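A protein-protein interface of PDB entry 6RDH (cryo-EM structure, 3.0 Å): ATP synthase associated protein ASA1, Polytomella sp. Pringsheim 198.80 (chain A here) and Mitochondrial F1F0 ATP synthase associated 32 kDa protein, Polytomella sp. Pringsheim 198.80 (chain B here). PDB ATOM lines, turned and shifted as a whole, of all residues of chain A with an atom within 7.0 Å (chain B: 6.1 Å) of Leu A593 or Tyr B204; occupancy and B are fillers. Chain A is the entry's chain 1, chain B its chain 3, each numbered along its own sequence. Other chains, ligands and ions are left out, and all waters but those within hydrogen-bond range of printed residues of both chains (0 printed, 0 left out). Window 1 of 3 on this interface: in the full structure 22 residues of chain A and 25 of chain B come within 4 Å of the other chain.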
ATOM      1  N   TRP A 521     -27.888 -12.767  24.937  1.00  0.00           N
ATOM      2  CA  TRP A 521     -27.825 -14.217  24.915  1.00  0.00           C
ATOM      3  C   TRP A 521     -27.987 -14.804  26.308  1.00  0.00           C
ATOM      4  O   TRP A 521     -28.763 -15.745  26.504  1.00  0.00           O
ATOM      5  CB  TRP A 521     -26.514 -14.647  24.295  1.00  0.00           C
ATOM      6  CG  TRP A 521     -26.242 -16.056  24.440  1.00  0.00           C
ATOM      7  CD1 TRP A 521     -26.904 -17.071  23.858  1.00  0.00           C
ATOM      8  CD2 TRP A 521     -25.207 -16.636  25.215  1.00  0.00           C
ATOM      9  NE1 TRP A 521     -26.354 -18.261  24.225  1.00  0.00           N
ATOM     10  CE2 TRP A 521     -25.301 -18.017  25.059  1.00  0.00           C
ATOM     11  CE3 TRP A 521     -24.201 -16.118  26.024  1.00  0.00           C
ATOM     12  CZ2 TRP A 521     -24.443 -18.887  25.682  1.00  0.00           C
ATOM     13  CZ3 TRP A 521     -23.351 -16.983  26.641  1.00  0.00           C
ATOM     14  CH2 TRP A 521     -23.471 -18.352  26.462  1.00  0.00           C
ATOM     15  N   LEU A 551     -34.656 -26.165  18.231  1.00  0.00           N
ATOM     16  CA  LEU A 551     -33.656 -27.138  17.828  1.00  0.00           C
ATOM     17  C   LEU A 551     -33.573 -28.301  18.794  1.00  0.00           C
ATOM     18  O   LEU A 551     -33.170 -29.389  18.392  1.00  0.00           O
ATOM     19  CB  LEU A 551     -32.293 -26.480  17.700  1.00  0.00           C
ATOM     20  CG  LEU A 551     -32.194 -25.327  16.726  1.00  0.00           C
ATOM     21  CD1 LEU A 551     -30.784 -24.868  16.703  1.00  0.00           C
ATOM     22  CD2 LEU A 551     -32.612 -25.776  15.375  1.00  0.00           C
ATOM     23  N   LYS A 555     -33.914 -32.107  17.523  1.00  0.00           N
ATOM     24  CA  LYS A 555     -33.042 -33.234  17.831  1.00  0.00           C
ATOM     25  C   LYS A 555     -33.802 -34.386  18.472  1.00  0.00           C
ATOM     26  O   LYS A 555     -33.518 -35.559  18.199  1.00  0.00           O
ATOM     27  CB  LYS A 555     -31.925 -32.777  18.745  1.00  0.00           C
ATOM     28  CG  LYS A 555     -31.041 -31.774  18.115  1.00  0.00           C
ATOM     29  CD  LYS A 555     -30.165 -31.152  19.129  1.00  0.00           C
ATOM     30  CE  LYS A 555     -29.351 -30.100  18.495  1.00  0.00           C
ATOM     31  NZ  LYS A 555     -28.251 -29.682  19.365  1.00  0.00           N
ATOM     32  N   GLU A 586     -24.916 -32.686  24.199  1.00  0.00           N
ATOM     33  CA  GLU A 586     -24.988 -32.488  22.763  1.00  0.00           C
ATOM     34  C   GLU A 586     -26.394 -32.192  22.291  1.00  0.00           C
ATOM     35  O   GLU A 586     -26.558 -31.692  21.177  1.00  0.00           O
ATOM     36  CB  GLU A 586     -24.482 -33.713  22.011  1.00  0.00           C
ATOM     37  CG  GLU A 586     -23.010 -33.983  22.116  1.00  0.00           C
ATOM     38  CD  GLU A 586     -22.175 -33.093  21.258  1.00  0.00           C
ATOM     39  OE1 GLU A 586     -22.718 -32.488  20.314  1.00  0.00           O
ATOM     40  OE2 GLU A 586     -20.961 -33.005  21.525  1.00  0.00           O
ATOM     41  N   ASN A 587     -27.415 -32.506  23.081  1.00  0.00           N
ATOM     42  CA  ASN A 587     -28.735 -32.051  22.680  1.00  0.00           C
ATOM     43  C   ASN A 587     -29.004 -30.618  23.086  1.00  0.00           C
ATOM     44  O   ASN A 587     -29.907 -29.994  22.530  1.00  0.00           O
ATOM     45  CB  ASN A 587     -29.819 -32.946  23.248  1.00  0.00           C
ATOM     46  CG  ASN A 587     -29.943 -34.237  22.500  1.00  0.00           C
ATOM     47  OD1 ASN A 587     -30.342 -35.251  23.050  1.00  0.00           O
ATOM     48  ND2 ASN A 587     -29.552 -34.219  21.245  1.00  0.00           N
ATOM     49  N   LEU A 588     -28.242 -30.080  24.029  1.00  0.00           N
ATOM     50  CA  LEU A 588     -28.332 -28.683  24.425  1.00  0.00           C
ATOM     51  C   LEU A 588     -27.097 -27.904  24.004  1.00  0.00           C
ATOM     52  O   LEU A 588     -26.707 -26.947  24.664  1.00  0.00           O
ATOM     53  CB  LEU A 588     -28.534 -28.571  25.928  1.00  0.00           C
ATOM     54  CG  LEU A 588     -29.779 -29.233  26.479  1.00  0.00           C
ATOM     55  CD1 LEU A 588     -29.736 -29.088  27.937  1.00  0.00           C
ATOM     56  CD2 LEU A 588     -30.983 -28.551  25.944  1.00  0.00           C
ATOM     57  N   SER A 589     -26.469 -28.312  22.913  1.00  0.00           N
ATOM     58  CA  SER A 589     -25.261 -27.668  22.437  1.00  0.00           C
ATOM     59  C   SER A 589     -25.544 -26.458  21.580  1.00  0.00           C
ATOM     60  O   SER A 589     -24.631 -25.677  21.316  1.00  0.00           O
ATOM     61  CB  SER A 589     -24.422 -28.651  21.629  1.00  0.00           C
ATOM     62  OG  SER A 589     -25.156 -29.125  20.521  1.00  0.00           O
ATOM     63  N   HIS A 590     -26.777 -26.291  21.135  1.00  0.00           N
ATOM     64  CA  HIS A 590     -27.166 -25.146  20.335  1.00  0.00           C
ATOM     65  C   HIS A 590     -27.440 -23.921  21.175  1.00  0.00           C
ATOM     66  O   HIS A 590     -27.756 -22.873  20.617  1.00  0.00           O
ATOM     67  CB  HIS A 590     -28.410 -25.473  19.524  1.00  0.00           C
ATOM     68  CG  HIS A 590     -29.530 -26.009  20.349  1.00  0.00           C
ATOM     69  ND1 HIS A 590     -30.586 -25.231  20.754  1.00  0.00           N
ATOM     70  CD2 HIS A 590     -29.752 -27.239  20.861  1.00  0.00           C
ATOM     71  CE1 HIS A 590     -31.413 -25.961  21.474  1.00  0.00           C
ATOM     72  NE2 HIS A 590     -30.926 -27.181  21.561  1.00  0.00           N
ATOM     73  N   HIS A 591     -27.366 -24.030  22.495  1.00  0.00           N
ATOM     74  CA  HIS A 591     -27.543 -22.861  23.336  1.00  0.00           C
ATOM     75  C   HIS A 591     -26.329 -21.961  23.284  1.00  0.00           C
ATOM     76  O   HIS A 591     -26.454 -20.746  23.440  1.00  0.00           O
ATOM     77  CB  HIS A 591     -27.819 -23.293  24.762  1.00  0.00           C
ATOM     78  CG  HIS A 591     -29.194 -23.831  24.965  1.00  0.00           C
ATOM     79  ND1 HIS A 591     -29.613 -24.376  26.153  1.00  0.00           N
ATOM     80  CD2 HIS A 591     -30.251 -23.893  24.129  1.00  0.00           C
ATOM     81  CE1 HIS A 591     -30.869 -24.760  26.038  1.00  0.00           C
ATOM     82  NE2 HIS A 591     -31.279 -24.479  24.818  1.00  0.00           N
ATOM     83  N   PHE A 592     -25.155 -22.532  23.072  1.00  0.00           N
ATOM     84  CA  PHE A 592     -23.927 -21.774  22.939  1.00  0.00           C
ATOM     85  C   PHE A 592     -23.596 -21.454  21.499  1.00  0.00           C
ATOM     86  O   PHE A 592     -22.528 -20.909  21.238  1.00  0.00           O
ATOM     87  CB  PHE A 592     -22.767 -22.539  23.560  1.00  0.00           C
ATOM     88  CG  PHE A 592     -23.053 -23.060  24.923  1.00  0.00           C
ATOM     89  CD1 PHE A 592     -22.935 -22.245  26.024  1.00  0.00           C
ATOM     90  CD2 PHE A 592     -23.433 -24.365  25.105  1.00  0.00           C
ATOM     91  CE1 PHE A 592     -23.199 -22.725  27.273  1.00  0.00           C
ATOM     92  CE2 PHE A 592     -23.695 -24.842  26.354  1.00  0.00           C
ATOM     93  CZ  PHE A 592     -23.576 -24.022  27.434  1.00  0.00           C
ATOM     94  N   LEU A 593     -24.451 -21.801  20.567  1.00  0.00           N
ATOM     95  CA  LEU A 593     -24.263 -21.410  19.178  1.00  0.00           C
ATOM     96  C   LEU A 593     -24.388 -19.905  18.913  1.00  0.00           C
ATOM     97  O   LEU A 593     -23.596 -19.399  18.105  1.00  0.00           O
ATOM     98  CB  LEU A 593     -25.223 -22.187  18.282  1.00  0.00           C
ATOM     99  CG  LEU A 593     -25.121 -21.922  16.791  1.00  0.00           C
ATOM    100  CD1 LEU A 593     -23.765 -22.306  16.314  1.00  0.00           C
ATOM    101  CD2 LEU A 593     -26.148 -22.696  16.076  1.00  0.00           C
ATOM    102  N   PRO A 594     -25.330 -19.145  19.517  1.00  0.00           N
ATOM    103  CA  PRO A 594     -25.290 -17.686  19.307  1.00  0.00           C
ATOM    104  C   PRO A 594     -24.021 -17.025  19.799  1.00  0.00           C
ATOM    105  O   PRO A 594     -23.482 -16.143  19.121  1.00  0.00           O
ATOM    106  CB  PRO A 594     -26.505 -17.199  20.094  1.00  0.00           C
ATOM    107  CG  PRO A 594     -27.401 -18.293  20.069  1.00  0.00           C
ATOM    108  CD  PRO A 594     -26.583 -19.491  20.218  1.00  0.00           C
ATOM    109  N   LEU A 595     -23.500 -17.481  20.933  1.00  0.00           N
ATOM    110  CA  LEU A 595     -22.276 -16.914  21.479  1.00  0.00           C
ATOM    111  C   LEU A 595     -21.082 -17.203  20.589  1.00  0.00           C
ATOM    112  O   LEU A 595     -20.298 -16.300  20.287  1.00  0.00           O
ATOM    113  CB  LEU A 595     -22.021 -17.460  22.870  1.00  0.00           C
ATOM    114  CG  LEU A 595     -20.719 -16.946  23.446  1.00  0.00           C
ATOM    115  CD1 LEU A 595     -20.858 -15.484  23.736  1.00  0.00           C
ATOM    116  CD2 LEU A 595     -20.367 -17.702  24.682  1.00  0.00           C
ATOM    117  N   ILE A 596     -20.919 -18.448  20.151  1.00  0.00           N
ATOM    118  CA  ILE A 596     -19.726 -18.737  19.373  1.00  0.00           C
ATOM    119  C   ILE A 596     -19.845 -18.234  17.948  1.00  0.00           C
ATOM    120  O   ILE A 596     -18.820 -17.929  17.339  1.00  0.00           O
ATOM    121  CB  ILE A 596     -19.366 -20.227  19.399  1.00  0.00           C
ATOM    122  CG1 ILE A 596     -20.401 -21.059  18.685  1.00  0.00           C
ATOM    123  CG2 ILE A 596     -19.227 -20.709  20.823  1.00  0.00           C
ATOM    124  CD1 ILE A 596     -19.993 -22.458  18.586  1.00  0.00           C
ATOM    125  N   ARG A 597     -21.053 -18.046  17.420  1.00  0.00           N
ATOM    126  CA  ARG A 597     -21.166 -17.361  16.139  1.00  0.00           C
ATOM    127  C   ARG A 597     -20.818 -15.884  16.267  1.00  0.00           C
ATOM    128  O   ARG A 597     -20.143 -15.324  15.394  1.00  0.00           O
ATOM    129  CB  ARG A 597     -22.568 -17.530  15.582  1.00  0.00           C
ATOM    130  CG  ARG A 597     -22.768 -18.834  14.912  1.00  0.00           C
ATOM    131  CD  ARG A 597     -24.207 -19.016  14.530  1.00  0.00           C
ATOM    132  NE  ARG A 597     -24.674 -18.014  13.593  1.00  0.00           N
ATOM    133  CZ  ARG A 597     -24.442 -18.051  12.289  1.00  0.00           C
ATOM    134  NH1 ARG A 597     -23.731 -19.033  11.756  1.00  0.00           N
ATOM    135  NH2 ARG A 597     -24.919 -17.093  11.515  1.00  0.00           N
ATOM    136  N   TYR A 598     -21.241 -15.245  17.364  1.00  0.00           N
ATOM    137  CA  TYR A 598     -20.877 -13.853  17.606  1.00  0.00           C
ATOM    138  C   TYR A 598     -19.380 -13.687  17.811  1.00  0.00           C
ATOM    139  O   TYR A 598     -18.778 -12.759  17.268  1.00  0.00           O
ATOM    140  CB  TYR A 598     -21.626 -13.324  18.817  1.00  0.00           C
ATOM    141  CG  TYR A 598     -21.122 -12.001  19.297  1.00  0.00           C
ATOM    142  CD1 TYR A 598     -21.194 -10.883  18.491  1.00  0.00           C
ATOM    143  CD2 TYR A 598     -20.590 -11.864  20.562  1.00  0.00           C
ATOM    144  CE1 TYR A 598     -20.742  -9.675  18.922  1.00  0.00           C
ATOM    145  CE2 TYR A 598     -20.136 -10.655  21.004  1.00  0.00           C
ATOM    146  CZ  TYR A 598     -20.218  -9.566  20.177  1.00  0.00           C
ATOM    147  OH  TYR A 598     -19.763  -8.349  20.599  1.00  0.00           O
ATOM    148  N   ARG A 599     -18.760 -14.582  18.569  1.00  0.00           N
ATOM    149  CA  ARG A 599     -17.334 -14.458  18.822  1.00  0.00           C
ATOM    150  C   ARG A 599     -16.509 -14.823  17.598  1.00  0.00           C
ATOM    151  O   ARG A 599     -15.435 -14.249  17.386  1.00  0.00           O
ATOM    152  CB  ARG A 599     -16.950 -15.318  20.012  1.00  0.00           C
ATOM    153  CG  ARG A 599     -17.502 -14.792  21.300  1.00  0.00           C
ATOM    154  CD  ARG A 599     -16.925 -15.522  22.472  1.00  0.00           C
ATOM    155  NE  ARG A 599     -17.368 -14.947  23.729  1.00  0.00           N
ATOM    156  CZ  ARG A 599     -17.019 -15.412  24.918  1.00  0.00           C
ATOM    157  NH1 ARG A 599     -16.223 -16.462  25.005  1.00  0.00           N
ATOM    158  NH2 ARG A 599     -17.463 -14.826  26.015  1.00  0.00           N
ATOM    159  N   ARG A 600     -17.008 -15.734  16.759  1.00  0.00           N
ATOM    160  CA  ARG A 600     -16.339 -16.029  15.501  1.00  0.00           C
ATOM    161  C   ARG A 600     -16.408 -14.844  14.554  1.00  0.00           C
ATOM    162  O   ARG A 600     -15.427 -14.534  13.874  1.00  0.00           O
ATOM    163  CB  ARG A 600     -16.961 -17.264  14.856  1.00  0.00           C
ATOM    164  CG  ARG A 600     -16.292 -17.695  13.571  1.00  0.00           C
ATOM    165  CD  ARG A 600     -16.945 -18.917  12.975  1.00  0.00           C
ATOM    166  NE  ARG A 600     -17.069 -19.982  13.954  1.00  0.00           N
ATOM    167  CZ  ARG A 600     -18.193 -20.642  14.191  1.00  0.00           C
ATOM    168  NH1 ARG A 600     -19.284 -20.354  13.503  1.00  0.00           N
ATOM    169  NH2 ARG A 600     -18.223 -21.595  15.105  1.00  0.00           N
ATOM    170  N   PRO A 612     -11.550 -21.833  19.758  1.00  0.00           N
ATOM    171  CA  PRO A 612     -12.111 -23.194  19.819  1.00  0.00           C
ATOM    172  C   PRO A 612     -12.425 -23.837  18.473  1.00  0.00           C
ATOM    173  O   PRO A 612     -12.698 -25.043  18.448  1.00  0.00           O
ATOM    174  CB  PRO A 612     -13.387 -23.000  20.636  1.00  0.00           C
ATOM    175  CG  PRO A 612     -13.080 -21.868  21.498  1.00  0.00           C
ATOM    176  CD  PRO A 612     -12.273 -20.935  20.672  1.00  0.00           C
ATOM    177  N   ASP A 613     -12.392 -23.100  17.364  1.00  0.00           N
ATOM    178  CA  ASP A 613     -12.583 -23.710  16.055  1.00  0.00           C
ATOM    179  C   ASP A 613     -11.344 -24.427  15.544  1.00  0.00           C
ATOM    180  O   ASP A 613     -11.398 -25.005  14.456  1.00  0.00           O
ATOM    181  CB  ASP A 613     -12.995 -22.659  15.028  1.00  0.00           C
ATOM    182  CG  ASP A 613     -14.372 -22.100  15.284  1.00  0.00           C
ATOM    183  OD1 ASP A 613     -15.010 -22.519  16.268  1.00  0.00           O
ATOM    184  OD2 ASP A 613     -14.817 -21.237  14.499  1.00  0.00           O
ATOM    185  N   PHE B 169     -29.849 -22.133   8.039  1.00  0.00           N
ATOM    186  CA  PHE B 169     -28.976 -23.248   8.376  1.00  0.00           C
ATOM    187  C   PHE B 169     -29.471 -24.028   9.582  1.00  0.00           C
ATOM    188  O   PHE B 169     -29.106 -25.191   9.740  1.00  0.00           O
ATOM    189  CB  PHE B 169     -27.550 -22.746   8.594  1.00  0.00           C
ATOM    190  CG  PHE B 169     -27.318 -22.127   9.932  1.00  0.00           C
ATOM    191  CD1 PHE B 169     -27.856 -20.900  10.247  1.00  0.00           C
ATOM    192  CD2 PHE B 169     -26.531 -22.762  10.868  1.00  0.00           C
ATOM    193  CE1 PHE B 169     -27.641 -20.344  11.467  1.00  0.00           C
ATOM    194  CE2 PHE B 169     -26.313 -22.204  12.086  1.00  0.00           C
ATOM    195  CZ  PHE B 169     -26.867 -20.996  12.385  1.00  0.00           C
ATOM    196  N   THR B 170     -30.329 -23.440  10.405  1.00  0.00           N
ATOM    197  CA  THR B 170     -30.852 -24.158  11.552  1.00  0.00           C
ATOM    198  C   THR B 170     -31.906 -25.181  11.169  1.00  0.00           C
ATOM    199  O   THR B 170     -32.230 -26.043  11.985  1.00  0.00           O
ATOM    200  CB  THR B 170     -31.440 -23.180  12.554  1.00  0.00           C
ATOM    201  OG1 THR B 170     -32.267 -22.247  11.864  1.00  0.00           O
ATOM    202  CG2 THR B 170     -30.357 -22.433  13.240  1.00  0.00           C
ATOM    203  N   ALA B 199     -21.000 -26.033   8.871  1.00  0.00           N
ATOM    204  CA  ALA B 199     -20.359 -26.656  10.021  1.00  0.00           C
ATOM    205  C   ALA B 199     -21.132 -26.379  11.299  1.00  0.00           C
ATOM    206  O   ALA B 199     -21.284 -27.274  12.140  1.00  0.00           O
ATOM    207  CB  ALA B 199     -18.923 -26.169  10.154  1.00  0.00           C
ATOM    208  N   ASP B 200     -21.666 -25.160  11.437  1.00  0.00           N
ATOM    209  CA  ASP B 200     -22.498 -24.820  12.585  1.00  0.00           C
ATOM    210  C   ASP B 200     -23.769 -25.645  12.598  1.00  0.00           C
ATOM    211  O   ASP B 200     -24.194 -26.115  13.653  1.00  0.00           O
ATOM    212  CB  ASP B 200     -22.851 -23.337  12.561  1.00  0.00           C
ATOM    213  CG  ASP B 200     -21.691 -22.452  12.938  1.00  0.00           C
ATOM    214  OD1 ASP B 200     -20.637 -22.977  13.348  1.00  0.00           O
ATOM    215  OD2 ASP B 200     -21.829 -21.219  12.810  1.00  0.00           O
ATOM    216  N   SER B 201     -24.353 -25.875  11.426  1.00  0.00           N
ATOM    217  CA  SER B 201     -25.593 -26.628  11.344  1.00  0.00           C
ATOM    218  C   SER B 201     -25.384 -28.092  11.694  1.00  0.00           C
ATOM    219  O   SER B 201     -26.098 -28.635  12.538  1.00  0.00           O
ATOM    220  CB  SER B 201     -26.177 -26.491   9.954  1.00  0.00           C
ATOM    221  OG  SER B 201     -27.404 -27.178   9.876  1.00  0.00           O
ATOM    222  N   ILE B 202     -24.386 -28.735  11.084  1.00  0.00           N
ATOM    223  CA  ILE B 202     -24.105 -30.142  11.355  1.00  0.00           C
ATOM    224  C   ILE B 202     -23.650 -30.346  12.794  1.00  0.00           C
ATOM    225  O   ILE B 202     -23.996 -31.353  13.423  1.00  0.00           O
ATOM    226  CB  ILE B 202     -23.076 -30.667  10.332  1.00  0.00           C
ATOM    227  CG1 ILE B 202     -23.705 -30.702   8.947  1.00  0.00           C
ATOM    228  CG2 ILE B 202     -22.558 -32.049  10.674  1.00  0.00           C
ATOM    229  CD1 ILE B 202     -22.809 -31.211   7.873  1.00  0.00           C
ATOM    230  N   THR B 203     -22.946 -29.377  13.374  1.00  0.00           N
ATOM    231  CA  THR B 203     -22.448 -29.596  14.722  1.00  0.00           C
ATOM    232  C   THR B 203     -23.515 -29.325  15.772  1.00  0.00           C
ATOM    233  O   THR B 203     -23.741 -30.149  16.662  1.00  0.00           O
ATOM    234  CB  THR B 203     -21.233 -28.720  14.972  1.00  0.00           C
ATOM    235  OG1 THR B 203     -20.297 -28.913  13.916  1.00  0.00           O
ATOM    236  CG2 THR B 203     -20.580 -29.119  16.263  1.00  0.00           C
ATOM    237  N   TYR B 204     -24.187 -28.177  15.687  1.00  0.00           N
ATOM    238  CA  TYR B 204     -25.041 -27.700  16.758  1.00  0.00           C
ATOM    239  C   TYR B 204     -26.521 -27.743  16.441  1.00  0.00           C
ATOM    240  O   TYR B 204     -27.322 -27.848  17.362  1.00  0.00           O
ATOM    241  CB  TYR B 204     -24.660 -26.263  17.129  1.00  0.00           C
ATOM    242  CG  TYR B 204     -23.208 -26.110  17.470  1.00  0.00           C
ATOM    243  CD1 TYR B 204     -22.732 -26.475  18.710  1.00  0.00           C
ATOM    244  CD2 TYR B 204     -22.310 -25.614  16.549  1.00  0.00           C
ATOM    245  CE1 TYR B 204     -21.413 -26.352  19.025  1.00  0.00           C
ATOM    246  CE2 TYR B 204     -20.984 -25.488  16.855  1.00  0.00           C
ATOM    247  CZ  TYR B 204     -20.542 -25.864  18.096  1.00  0.00           C
ATOM    248  OH  TYR B 204     -19.217 -25.741  18.417  1.00  0.00           O
ATOM    249  N   CYS B 205     -26.917 -27.657  15.182  1.00  0.00           N
ATOM    250  CA  CYS B 205     -28.328 -27.597  14.864  1.00  0.00           C
ATOM    251  C   CYS B 205     -28.922 -28.953  14.549  1.00  0.00           C
ATOM    252  O   CYS B 205     -30.127 -29.040  14.316  1.00  0.00           O
ATOM    253  CB  CYS B 205     -28.555 -26.662  13.685  1.00  0.00           C
ATOM    254  SG  CYS B 205     -27.863 -25.043  13.926  1.00  0.00           S
ATOM    255  N   ASN B 206     -28.115 -30.002  14.517  1.00  0.00           N
ATOM    256  CA  ASN B 206     -28.581 -31.340  14.207  1.00  0.00           C
ATOM    257  C   ASN B 206     -28.155 -32.279  15.315  1.00  0.00           C
ATOM    258  O   ASN B 206     -27.360 -31.925  16.183  1.00  0.00           O
ATOM    259  CB  ASN B 206     -28.041 -31.826  12.865  1.00  0.00           C
ATOM    260  CG  ASN B 206     -28.551 -31.011  11.714  1.00  0.00           C
ATOM    261  OD1 ASN B 206     -27.885 -30.858  10.705  1.00  0.00           O
ATOM    262  ND2 ASN B 206     -29.733 -30.472  11.861  1.00  0.00           N
ATOM    263  N   ARG B 233     -12.251 -26.702  11.259  1.00  0.00           N
ATOM    264  CA  ARG B 233     -13.388 -26.611  12.175  1.00  0.00           C
ATOM    265  C   ARG B 233     -13.334 -27.872  13.029  1.00  0.00           C
ATOM    266  O   ARG B 233     -13.907 -28.885  12.640  1.00  0.00           O
ATOM    267  CB  ARG B 233     -14.702 -26.521  11.415  1.00  0.00           C
ATOM    268  CG  ARG B 233     -14.970 -25.207  10.733  1.00  0.00           C
ATOM    269  CD  ARG B 233     -15.187 -24.125  11.746  1.00  0.00           C
ATOM    270  NE  ARG B 233     -16.140 -24.542  12.759  1.00  0.00           N
ATOM    271  CZ  ARG B 233     -17.413 -24.176  12.782  1.00  0.00           C
ATOM    272  NH1 ARG B 233     -18.207 -24.607  13.746  1.00  0.00           N
ATOM    273  NH2 ARG B 233     -17.885 -23.370  11.851  1.00  0.00           N
ATOM    274  N   ASP B 235     -14.701 -28.716  15.799  1.00  0.00           N
ATOM    275  CA  ASP B 235     -16.000 -29.188  16.262  1.00  0.00           C
ATOM    276  C   ASP B 235     -16.681 -30.038  15.198  1.00  0.00           C
ATOM    277  O   ASP B 235     -17.184 -31.131  15.491  1.00  0.00           O
ATOM    278  CB  ASP B 235     -16.861 -27.990  16.656  1.00  0.00           C
ATOM    279  CG  ASP B 235     -16.771 -26.851  15.655  1.00  0.00           C
ATOM    280  OD1 ASP B 235     -16.134 -27.032  14.608  1.00  0.00           O
ATOM    281  OD2 ASP B 235     -17.311 -25.763  15.925  1.00  0.00           O
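NH1 of Arg A600 lies within salt-bridge range of OD2 of Asp B200 (2.8 Å).
OD2 of Asp A613 lies within salt-bridge range of NE of Arg B233.
NH1 of Arg A597 lies within salt-bridge range of OD2 of Asp B200 (3.1 Å).
NH1 of Arg B233 sits close to NH2 of Arg A600 (3.3 Å).
O of Tyr B204 is in hydrogen-bond range of NZ of Lys A555 (2.9 Å).
The backbone carbonyl oxygen of Asp B200 is in hydrogen-bond range of the backbone NH of Cys B205, at 3.5 Å.
O of Phe B169 lies within hydrogen-bond range of OG of Ser B201, 2.6 Å away.
The backbone carbonyl oxygen (O) of Ser B201 lies within hydrogen-bond range of the backbone NH (N) of Asn B206, 3.1 Å away.
The guanidinium group (NE) of Arg A600 is in salt-bridge range of the side-chain carboxylate (OD2) of Asp A613, at 2.6 Å.
NH1 of Arg B233 lies within salt-bridge range of OD2 of Asp B235 (2.6 Å).
The side-chain carboxylate (OD1) of Asp B200 lies within salt-bridge range of the guanidinium group (NH1) of Arg B233, at 3.0 Å.
Among the printed residues, merely in contact across the chains: Leu A551 with Thr B170, Lys A555 with Asn B206, Ser A589 with Tyr B204, His A590 with Tyr B204, Leu A593 with Asp B200, Leu A593 with Tyr B204, Leu A593 with Cys B205, Ile A596 with Tyr B204, Arg A597 with Phe B169 and Asp A613 with Asp B235.
Leu A593 touches just these residues of chain B: Asp B200 (3.96 Å), Tyr B204 (3.6 Å) and Cys B205 (3.6 Å).
Tyr B204 touches just these residues of chain A: Lys A555, Ser A589, His A590, Leu A593 and Ile A596.
Printed residues of chain B within 4 Å of Lys A555: Tyr B204 (2.9 Å) and Asn B206 (3.6 Å).
Of the printed residues of chain A, Thr B170 touches Leu A551.
Of the printed residues of chain A, Arg B233 touches Arg A600 (3.3 Å) and Asp A613 (3.4 Å).
Of the printed residues of chain B, His A590 touches Tyr B204.
Printed residues of chain A within 4 Å of Asp B235: Asp A613 (3.99 Å).
The nearest printed residue of chain B that does not touch Ile A596 is Asp B235 (5.0 Å).
Printed residues of chain A that touch a printed residue of chain B: Leu A551, Lys A555, Ser A589, His A590, Leu A593, Ile A596, Arg A597, Arg A600 and Asp A613.
Hydrophobic or aromatic side chains of chain A within 4 Å of the printed part of chain B: Leu A551, His A590, Leu A593 and Ile A596.
Along chain A the printed residues that touch a printed residue of chain B span positions 551 to 613.
Of the 12 printed residues of chain B, 8 touch a printed residue of chain A.
Hydrophobic or aromatic side chains of chain B within 4 Å of the printed part of chain A: Phe B169 and Tyr B204.
Among the printed residues, 15 pairs touch across the chains.
Among the printed residues, Asp or Glu carboxylates within 4 Å of a Lys or Arg side-chain nitrogen of the other chain: Arg A597 with Asp B200 (3.1 Å), Arg A600 with Asp B200 (2.8 Å) and Asp A613 with Arg B233 (3.96 Å).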
